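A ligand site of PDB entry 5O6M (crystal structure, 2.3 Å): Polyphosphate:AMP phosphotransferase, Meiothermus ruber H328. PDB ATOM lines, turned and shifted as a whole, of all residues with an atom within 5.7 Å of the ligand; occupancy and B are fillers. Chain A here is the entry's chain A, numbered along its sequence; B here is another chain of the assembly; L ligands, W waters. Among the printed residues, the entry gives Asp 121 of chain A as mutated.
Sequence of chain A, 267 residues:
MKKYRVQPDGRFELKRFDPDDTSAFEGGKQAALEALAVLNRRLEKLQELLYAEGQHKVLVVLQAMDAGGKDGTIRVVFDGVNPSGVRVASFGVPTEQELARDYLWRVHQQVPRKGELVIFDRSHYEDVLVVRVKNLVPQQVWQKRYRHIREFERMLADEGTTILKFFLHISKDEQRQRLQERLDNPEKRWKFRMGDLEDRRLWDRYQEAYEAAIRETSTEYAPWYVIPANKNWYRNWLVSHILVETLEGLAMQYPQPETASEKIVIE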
ATOM      1  N   ASP A  66     -30.123 -16.310 -10.146  1.00  0.00           N
ATOM      2  CA  ASP A  66     -29.124 -15.324 -10.532  1.00  0.00           C
ATOM      3  C   ASP A  66     -29.279 -14.043  -9.707  1.00  0.00           C
ATOM      4  O   ASP A  66     -30.398 -13.573  -9.464  1.00  0.00           O
ATOM      5  CB  ASP A  66     -29.244 -14.996 -12.026  1.00  0.00           C
ATOM      6  CG  ASP A  66     -29.013 -16.209 -12.902  1.00  0.00           C
ATOM      7  OD1 ASP A  66     -29.570 -16.235 -14.022  1.00  0.00           O
ATOM      8  OD2 ASP A  66     -28.307 -17.141 -12.468  1.00  0.00           O
ATOM      9  N   LYS A  70     -24.821 -15.261  -4.056  1.00  0.00           N
ATOM     10  CA  LYS A  70     -23.784 -16.266  -3.838  1.00  0.00           C
ATOM     11  C   LYS A  70     -22.428 -15.609  -3.622  1.00  0.00           C
ATOM     12  O   LYS A  70     -21.694 -15.969  -2.687  1.00  0.00           O
ATOM     13  CB  LYS A  70     -23.707 -17.229  -5.030  1.00  0.00           C
ATOM     14  CG  LYS A  70     -24.908 -18.126  -5.238  1.00  0.00           C
ATOM     15  CD  LYS A  70     -24.657 -19.161  -6.356  1.00  0.00           C
ATOM     16  CE  LYS A  70     -24.550 -18.516  -7.741  1.00  0.00           C
ATOM     17  NZ  LYS A  70     -23.152 -18.157  -8.117  1.00  0.00           N
ATOM     18  N   SER A  90     -15.923 -23.255  -8.316  1.00  0.00           N
ATOM     19  CA  SER A  90     -17.017 -22.746  -9.134  1.00  0.00           C
ATOM     20  C   SER A  90     -17.315 -23.705 -10.269  1.00  0.00           C
ATOM     21  O   SER A  90     -16.398 -24.312 -10.848  1.00  0.00           O
ATOM     22  CB  SER A  90     -16.666 -21.367  -9.703  1.00  0.00           C
ATOM     23  OG  SER A  90     -16.484 -20.423  -8.678  1.00  0.00           O
ATOM     24  N   PHE A  91     -18.596 -23.844 -10.593  1.00  0.00           N
ATOM     25  CA  PHE A  91     -19.048 -24.702 -11.676  1.00  0.00           C
ATOM     26  C   PHE A  91     -19.837 -23.856 -12.667  1.00  0.00           C
ATOM     27  O   PHE A  91     -20.885 -23.314 -12.317  1.00  0.00           O
ATOM     28  CB  PHE A  91     -19.882 -25.861 -11.125  1.00  0.00           C
ATOM     29  CG  PHE A  91     -19.106 -26.774 -10.238  1.00  0.00           C
ATOM     30  CD1 PHE A  91     -18.271 -27.753 -10.775  1.00  0.00           C
ATOM     31  CD2 PHE A  91     -19.169 -26.641  -8.861  1.00  0.00           C
ATOM     32  CE1 PHE A  91     -17.533 -28.591  -9.947  1.00  0.00           C
ATOM     33  CE2 PHE A  91     -18.437 -27.467  -8.031  1.00  0.00           C
ATOM     34  CZ  PHE A  91     -17.617 -28.444  -8.572  1.00  0.00           C
ATOM     35  N   GLY A  92     -19.317 -23.737 -13.888  1.00  0.00           N
ATOM     36  CA  GLY A  92     -19.991 -23.003 -14.925  1.00  0.00           C
ATOM     37  C   GLY A  92     -20.521 -23.890 -16.033  1.00  0.00           C
ATOM     38  O   GLY A  92     -20.885 -25.043 -15.793  1.00  0.00           O
ATOM     39  N   VAL A  93     -20.593 -23.353 -17.249  1.00  0.00           N
ATOM     40  CA  VAL A  93     -21.037 -24.170 -18.382  1.00  0.00           C
ATOM     41  C   VAL A  93     -20.084 -25.350 -18.559  1.00  0.00           C
ATOM     42  O   VAL A  93     -18.858 -25.140 -18.646  1.00  0.00           O
ATOM     43  CB  VAL A  93     -21.108 -23.324 -19.661  1.00  0.00           C
ATOM     44  CG1 VAL A  93     -21.524 -24.185 -20.845  1.00  0.00           C
ATOM     45  CG2 VAL A  93     -22.082 -22.163 -19.468  1.00  0.00           C
ATOM     46  N   PRO A  94     -20.563 -26.587 -18.597  1.00  0.00           N
ATOM     47  CA  PRO A  94     -19.660 -27.730 -18.759  1.00  0.00           C
ATOM     48  C   PRO A  94     -18.906 -27.666 -20.077  1.00  0.00           C
ATOM     49  O   PRO A  94     -19.457 -27.292 -21.111  1.00  0.00           O
ATOM     50  CB  PRO A  94     -20.599 -28.944 -18.715  1.00  0.00           C
ATOM     51  CG  PRO A  94     -21.786 -28.470 -17.927  1.00  0.00           C
ATOM     52  CD  PRO A  94     -21.941 -27.001 -18.276  1.00  0.00           C
ATOM     53  N   ARG A 106     -16.857 -34.001 -12.819  1.00  0.00           N
ATOM     54  CA  ARG A 106     -16.183 -32.730 -12.556  1.00  0.00           C
ATOM     55  C   ARG A 106     -16.454 -32.220 -11.155  1.00  0.00           C
ATOM     56  O   ARG A 106     -15.650 -31.453 -10.622  1.00  0.00           O
ATOM     57  CB  ARG A 106     -16.616 -31.686 -13.586  1.00  0.00           C
ATOM     58  CG  ARG A 106     -18.061 -31.250 -13.435  1.00  0.00           C
ATOM     59  CD  ARG A 106     -18.356 -30.029 -14.281  1.00  0.00           C
ATOM     60  NE  ARG A 106     -19.662 -29.450 -13.998  1.00  0.00           N
ATOM     61  CZ  ARG A 106     -20.034 -28.232 -14.365  1.00  0.00           C
ATOM     62  NH1 ARG A 106     -19.196 -27.454 -15.044  1.00  0.00           N
ATOM     63  NH2 ARG A 106     -21.254 -27.785 -14.072  1.00  0.00           N
ATOM     64  N   ASP A 121     -19.534 -23.075  -5.335  1.00  0.00           N
ATOM     65  CA  ASP A 121     -20.223 -21.913  -5.907  1.00  0.00           C
ATOM     66  C   ASP A 121     -20.973 -22.429  -7.136  1.00  0.00           C
ATOM     67  O   ASP A 121     -20.420 -22.569  -8.227  1.00  0.00           O
ATOM     68  CB  ASP A 121     -19.215 -20.811  -6.222  1.00  0.00           C
ATOM     69  CG  ASP A 121     -19.782 -19.710  -7.076  1.00  0.00           C
ATOM     70  OD1 ASP A 121     -18.984 -19.039  -7.759  1.00  0.00           O
ATOM     71  OD2 ASP A 121     -21.010 -19.494  -7.051  1.00  0.00           O
ATOM     72  N   ARG A 122     -22.253 -22.766  -6.927  1.00  0.00           N
ATOM     73  CA  ARG A 122     -22.989 -23.659  -7.825  1.00  0.00           C
ATOM     74  C   ARG A 122     -22.393 -25.054  -7.663  1.00  0.00           C
ATOM     75  O   ARG A 122     -21.320 -25.198  -7.083  1.00  0.00           O
ATOM     76  CB  ARG A 122     -22.944 -23.182  -9.269  1.00  0.00           C
ATOM     77  CG  ARG A 122     -23.738 -21.887  -9.502  1.00  0.00           C
ATOM     78  CD  ARG A 122     -23.831 -21.555 -10.982  1.00  0.00           C
ATOM     79  NE  ARG A 122     -24.335 -20.201 -11.216  1.00  0.00           N
ATOM     80  CZ  ARG A 122     -25.622 -19.890 -11.311  1.00  0.00           C
ATOM     81  NH1 ARG A 122     -26.544 -20.841 -11.191  1.00  0.00           N
ATOM     82  NH2 ARG A 122     -25.995 -18.633 -11.523  1.00  0.00           N
ATOM     83  N   SER A 123     -23.082 -26.094  -8.151  1.00  0.00           N
ATOM     84  CA  SER A 123     -22.699 -27.452  -7.764  1.00  0.00           C
ATOM     85  C   SER A 123     -23.297 -28.458  -8.746  1.00  0.00           C
ATOM     86  O   SER A 123     -23.788 -28.090  -9.821  1.00  0.00           O
ATOM     87  CB  SER A 123     -23.199 -27.772  -6.358  1.00  0.00           C
ATOM     88  OG  SER A 123     -24.615 -27.853  -6.372  1.00  0.00           O
ATOM     89  N   GLU A 126     -26.930 -28.041 -10.364  1.00  0.00           N
ATOM     90  CA  GLU A 126     -27.233 -27.467 -11.670  1.00  0.00           C
ATOM     91  C   GLU A 126     -27.692 -28.537 -12.656  1.00  0.00           C
ATOM     92  O   GLU A 126     -28.401 -28.219 -13.620  1.00  0.00           O
ATOM     93  CB  GLU A 126     -26.020 -26.722 -12.217  1.00  0.00           C
ATOM     94  CG  GLU A 126     -25.592 -25.507 -11.393  1.00  0.00           C
ATOM     95  CD  GLU A 126     -26.575 -24.344 -11.489  1.00  0.00           C
ATOM     96  OE1 GLU A 126     -27.277 -24.238 -12.516  1.00  0.00           O
ATOM     97  OE2 GLU A 126     -26.620 -23.514 -10.539  1.00  0.00           O
ATOM     98  N   ASP A 127     -27.296 -29.799 -12.451  1.00  0.00           N
ATOM     99  CA  ASP A 127     -27.685 -30.875 -13.356  1.00  0.00           C
ATOM    100  C   ASP A 127     -29.103 -31.390 -13.098  1.00  0.00           C
ATOM    101  O   ASP A 127     -29.531 -32.317 -13.790  1.00  0.00           O
ATOM    102  CB  ASP A 127     -26.681 -32.027 -13.253  1.00  0.00           C
ATOM    103  CG  ASP A 127     -25.333 -31.662 -13.859  1.00  0.00           C
ATOM    104  OD1 ASP A 127     -25.258 -31.525 -15.100  1.00  0.00           O
ATOM    105  OD2 ASP A 127     -24.357 -31.507 -13.101  1.00  0.00           O
ATOM    106  N   VAL A 130     -30.803 -26.003 -14.094  1.00  0.00           N
ATOM    107  CA  VAL A 130     -30.742 -25.479 -15.456  1.00  0.00           C
ATOM    108  C   VAL A 130     -30.903 -26.612 -16.470  1.00  0.00           C
ATOM    109  O   VAL A 130     -31.511 -26.432 -17.526  1.00  0.00           O
ATOM    110  CB  VAL A 130     -29.425 -24.709 -15.674  1.00  0.00           C
ATOM    111  CG1 VAL A 130     -28.240 -25.639 -15.465  1.00  0.00           C
ATOM    112  CG2 VAL A 130     -29.401 -24.083 -17.053  1.00  0.00           C
ATOM    113  N   VAL A 131     -30.346 -27.795 -16.166  1.00  0.00           N
ATOM    114  CA  VAL A 131     -30.453 -28.919 -17.086  1.00  0.00           C
ATOM    115  C   VAL A 131     -31.909 -29.327 -17.269  1.00  0.00           C
ATOM    116  O   VAL A 131     -32.346 -29.652 -18.374  1.00  0.00           O
ATOM    117  CB  VAL A 131     -29.594 -30.105 -16.606  1.00  0.00           C
ATOM    118  CG1 VAL A 131     -30.001 -31.376 -17.321  1.00  0.00           C
ATOM    119  CG2 VAL A 131     -28.105 -29.805 -16.822  1.00  0.00           C
ATOM    120  N   LEU A 136     -31.790 -29.860 -21.273  1.00  0.00           N
ATOM    121  CA  LEU A 136     -30.493 -30.182 -21.860  1.00  0.00           C
ATOM    122  C   LEU A 136     -30.302 -31.688 -21.961  1.00  0.00           C
ATOM    123  O   LEU A 136     -29.451 -32.149 -22.735  1.00  0.00           O
ATOM    124  CB  LEU A 136     -29.382 -29.539 -21.025  1.00  0.00           C
ATOM    125  CG  LEU A 136     -29.506 -28.003 -20.956  1.00  0.00           C
ATOM    126  CD1 LEU A 136     -28.335 -27.370 -20.200  1.00  0.00           C
ATOM    127  CD2 LEU A 136     -29.618 -27.403 -22.355  1.00  0.00           C
ATOM    128  N   ARG A 182     -27.370  -3.792 -11.370  1.00  0.00           N
ATOM    129  CA  ARG A 182     -26.219  -4.298 -12.107  1.00  0.00           C
ATOM    130  C   ARG A 182     -26.059  -3.584 -13.439  1.00  0.00           C
ATOM    131  O   ARG A 182     -24.927  -3.382 -13.897  1.00  0.00           O
ATOM    132  CB  ARG A 182     -26.356  -5.815 -12.308  1.00  0.00           C
ATOM    133  CG  ARG A 182     -25.133  -6.599 -11.873  1.00  0.00           C
ATOM    134  CD  ARG A 182     -25.492  -7.695 -10.871  1.00  0.00           C
ATOM    135  NE  ARG A 182     -25.536  -9.008 -11.502  1.00  0.00           N
ATOM    136  CZ  ARG A 182     -25.453 -10.164 -10.850  1.00  0.00           C
ATOM    137  NH1 ARG A 182     -25.495 -11.306 -11.515  1.00  0.00           N
ATOM    138  NH2 ARG A 182     -25.307 -10.174  -9.533  1.00  0.00           N
ATOM    139  N   LYS A 191     -20.876  -7.926 -14.544  1.00  0.00           N
ATOM    140  CA  LYS A 191     -21.595  -9.065 -14.010  1.00  0.00           C
ATOM    141  C   LYS A 191     -22.849  -9.401 -14.816  1.00  0.00           C
ATOM    142  O   LYS A 191     -23.324 -10.535 -14.756  1.00  0.00           O
ATOM    143  CB  LYS A 191     -22.011  -8.807 -12.562  1.00  0.00           C
ATOM    144  CG  LYS A 191     -20.886  -8.709 -11.543  1.00  0.00           C
ATOM    145  CD  LYS A 191     -21.409  -8.141 -10.227  1.00  0.00           C
ATOM    146  CE  LYS A 191     -20.419  -8.330  -9.087  1.00  0.00           C
ATOM    147  NZ  LYS A 191     -20.349  -9.742  -8.624  1.00  0.00           N
ATOM    148  N   ASP A 199     -33.041 -16.334 -18.474  1.00  0.00           N
ATOM    149  CA  ASP A 199     -33.249 -17.093 -17.243  1.00  0.00           C
ATOM    150  C   ASP A 199     -34.356 -16.482 -16.393  1.00  0.00           C
ATOM    151  O   ASP A 199     -35.110 -17.214 -15.744  1.00  0.00           O
ATOM    152  CB  ASP A 199     -31.949 -17.178 -16.443  1.00  0.00           C
ATOM    153  CG  ASP A 199     -30.939 -18.123 -17.070  1.00  0.00           C
ATOM    154  OD1 ASP A 199     -31.352 -19.065 -17.773  1.00  0.00           O
ATOM    155  OD2 ASP A 199     -29.719 -17.933 -16.841  1.00  0.00           O
ATOM    156  N   TYR A 206     -37.588 -22.373 -12.874  1.00  0.00           N
ATOM    157  CA  TYR A 206     -36.476 -22.534 -11.948  1.00  0.00           C
ATOM    158  C   TYR A 206     -36.977 -22.753 -10.525  1.00  0.00           C
ATOM    159  O   TYR A 206     -36.488 -23.648  -9.813  1.00  0.00           O
ATOM    160  CB  TYR A 206     -35.541 -21.321 -12.006  1.00  0.00           C
ATOM    161  CG  TYR A 206     -34.467 -21.417 -13.069  1.00  0.00           C
ATOM    162  CD1 TYR A 206     -34.503 -20.624 -14.200  1.00  0.00           C
ATOM    163  CD2 TYR A 206     -33.401 -22.304 -12.928  1.00  0.00           C
ATOM    164  CE1 TYR A 206     -33.520 -20.712 -15.174  1.00  0.00           C
ATOM    165  CE2 TYR A 206     -32.408 -22.397 -13.882  1.00  0.00           C
ATOM    166  CZ  TYR A 206     -32.481 -21.600 -15.009  1.00  0.00           C
ATOM    167  OH  TYR A 206     -31.500 -21.674 -15.968  1.00  0.00           O
ATOM    168  N   TYR B  51      -9.903  -9.866 -10.710  1.00  0.00           N
ATOM    169  CA  TYR B  51     -10.910 -10.884 -10.960  1.00  0.00           C
ATOM    170  C   TYR B  51     -11.910 -10.430 -12.030  1.00  0.00           C
ATOM    171  O   TYR B  51     -12.216 -11.175 -12.966  1.00  0.00           O
ATOM    172  CB  TYR B  51     -11.631 -11.210  -9.645  1.00  0.00           C
ATOM    173  CG  TYR B  51     -12.587 -12.370  -9.732  1.00  0.00           C
ATOM    174  CD1 TYR B  51     -13.954 -12.161  -9.773  1.00  0.00           C
ATOM    175  CD2 TYR B  51     -12.120 -13.685  -9.742  1.00  0.00           C
ATOM    176  CE1 TYR B  51     -14.837 -13.223  -9.844  1.00  0.00           C
ATOM    177  CE2 TYR B  51     -12.998 -14.753  -9.807  1.00  0.00           C
ATOM    178  CZ  TYR B  51     -14.360 -14.516  -9.858  1.00  0.00           C
ATOM    179  OH  TYR B  51     -15.236 -15.567  -9.926  1.00  0.00           O
HETATM  180  P1  LIG L   1     -22.500 -16.843 -11.749  1.00  0.00           P
HETATM  181  O1  LIG L   1     -21.841 -15.819 -10.870  1.00  0.00           O
HETATM  182  O2  LIG L   1     -24.017 -16.716 -11.802  1.00  0.00           O
HETATM  183  O3  LIG L   1     -22.158 -18.295 -11.351  1.00  0.00           O
HETATM  184  P2  LIG L   1     -20.678 -16.251 -13.978  1.00  0.00           P
HETATM  185  O4  LIG L   1     -20.856 -15.065 -14.847  1.00  0.00           O
HETATM  186  O5  LIG L   1     -19.618 -16.145 -12.894  1.00  0.00           O
HETATM  187  O6  LIG L   1     -22.047 -16.662 -13.265  1.00  0.00           O
HETATM  188  P3  LIG L   1     -20.057 -19.068 -14.449  1.00  0.00           P
HETATM  189  O7  LIG L   1     -19.582 -19.199 -13.062  1.00  0.00           O
HETATM  190  O8  LIG L   1     -19.061 -19.569 -15.508  1.00  0.00           O
HETATM  191  O9  LIG L   1     -20.359 -17.549 -14.834  1.00  0.00           O
HETATM  192  O10 LIG L   1     -21.466 -19.869 -14.662  1.00  0.00           O
HETATM  193  C1  LIG L   1     -22.263 -19.542 -15.821  1.00  0.00           C
HETATM  194  C2  LIG L   1     -23.421 -20.483 -16.011  1.00  0.00           C
HETATM  195  O11 LIG L   1     -23.031 -21.864 -15.901  1.00  0.00           O
HETATM  196  C3  LIG L   1     -24.615 -20.308 -15.062  1.00  0.00           C
HETATM  197  O12 LIG L   1     -25.694 -19.679 -15.758  1.00  0.00           O
HETATM  198  C4  LIG L   1     -25.001 -21.756 -14.693  1.00  0.00           C
HETATM  199  O13 LIG L   1     -26.402 -22.010 -14.792  1.00  0.00           O
HETATM  200  C5  LIG L   1     -24.257 -22.549 -15.763  1.00  0.00           C
HETATM  201  N1  LIG L   1     -24.039 -23.951 -15.439  1.00  0.00           N
HETATM  202  C6  LIG L   1     -23.513 -24.476 -14.299  1.00  0.00           C
HETATM  203  N2  LIG L   1     -23.602 -25.784 -14.223  1.00  0.00           N
HETATM  204  C7  LIG L   1     -24.230 -26.140 -15.404  1.00  0.00           C
HETATM  205  C8  LIG L   1     -24.640 -27.386 -15.927  1.00  0.00           C
HETATM  206  N3  LIG L   1     -24.466 -28.549 -15.297  1.00  0.00           N
HETATM  207  N4  LIG L   1     -25.241 -27.392 -17.138  1.00  0.00           N
HETATM  208  C9  LIG L   1     -25.415 -26.229 -17.768  1.00  0.00           C
HETATM  209  N5  LIG L   1     -25.080 -24.998 -17.377  1.00  0.00           N
HETATM  210  C10 LIG L   1     -24.493 -25.022 -16.181  1.00  0.00           C
HETATM  211  O   HOH W   1     -19.538 -20.601 -17.847  1.00  0.00           O
HETATM  212  O   HOH W   2     -29.320 -21.848 -13.916  1.00  0.00           O
HETATM  213  O   HOH W   3     -24.061 -31.279 -17.230  1.00  0.00           O
HETATM  214  O   HOH W   4     -23.070 -29.083 -12.355  1.00  0.00           O
HETATM  215  O   HOH W   5     -24.995 -29.446 -18.932  1.00  0.00           O
HETATM  216  O   HOH W   6     -25.694 -15.780  -9.732  1.00  0.00           O
HETATM  217  O   HOH W   7     -20.472 -20.873 -10.464  1.00  0.00           O
HETATM  218  O   HOH W   8     -24.956 -16.127 -14.450  1.00  0.00           O
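OE1 of Glu 126 sits at hydrogen-bond distance from O13 of the ligand (3.3 Å).
The guanidinium group (NH2) of Arg 122 lies within salt-bridge range of an oxygen (O2) of the ligand (2.8 Å).
O11 of the ligand is in hydrogen-bond range of N of Val 93 (3.2 Å).
NZ of Lys 70 is in salt-bridge range of O3 of the ligand (3.4 Å).
The guanidinium group (NH2) of Arg 106 sits at hydrogen-bond distance from a nitrogen (N2) of the ligand (3.1 Å).
OD1 of Asp 127 lies within hydrogen-bond range of N3 of the ligand.
O of Val 131 is in hydrogen-bond range of N of Leu 136, 3.0 Å away.
NH1 of Arg 106 is in hydrogen-bond range of O of Gly 92, 3.0 Å away.
The side-chain carboxylate (OD2) of Asp 66 lies within salt-bridge range of the guanidinium group (NH2) of Arg 122 (2.9 Å).
The backbone carbonyl oxygen (O) of Glu 126 sits at hydrogen-bond distance from the backbone NH (N) of Val 131 (3.2 Å).
The backbone NH (N) of Phe 91 is in hydrogen-bond range of the backbone carbonyl oxygen (O) of Asp 121 (3.2 Å).
The guanidinium group of Arg 122 is in salt-bridge range of the side-chain carboxylate of Glu 126, 2.8 Å away.
OD2 of Asp 121 lies within salt-bridge range of NZ of Lys 70 (2.7 Å).
N2 of the ligand lies close to O of Gly 92.
Phe 91 touches the ligand.
Pro 94 touches the ligand.
Val 130 touches the ligand (CG1 to C9, 3.7 Å).
Val 131 touches the ligand.
CD1 of Leu 136 touches C9 of the ligand, at 3.97 Å.
Hydrophobic or aromatic side chains that line the ligand: Val 93, Pro 94, Val 130, Val 131 and Leu 136.
Within 4 Å of the ligand: Lys 70, Phe 91, Gly 92, Val 93, Pro 94, Arg 106, Arg 122, Glu 126, Asp 127, Val 130, Val 131 and Leu 136.
The nearest printed residue that does not touch the ligand is Asp 66 (4.4 Å).
Water W1 bridges O8 of the ligand (2.6 Å) and N of Val 93 (3.0 Å).
Water W6 bridges an oxygen (O2) of the ligand (2.8 Å) and the guanidinium group of Arg 122 (3.4 Å).
Water W2 lies within hydrogen-bond range of OH of Tyr 206 (3.0 Å), O13 of the ligand (3.1 Å) and OE1 of Glu 126 (3.4 Å).
Water W7 lies within hydrogen-bond range of O of Asp 121, O of Phe 91 and O3 of the ligand.
Water W4 lies within hydrogen-bond range of the backbone carbonyl oxygen of Ser 123 (2.8 Å), the guanidinium group of Arg 106 (2.8 Å), the side-chain carboxylate of Asp 127 (2.8 Å) and a nitrogen (N3) of the ligand (3.3 Å).
Water W3 lies within hydrogen-bond range of OD1 of Asp 127 and N3 of the ligand.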
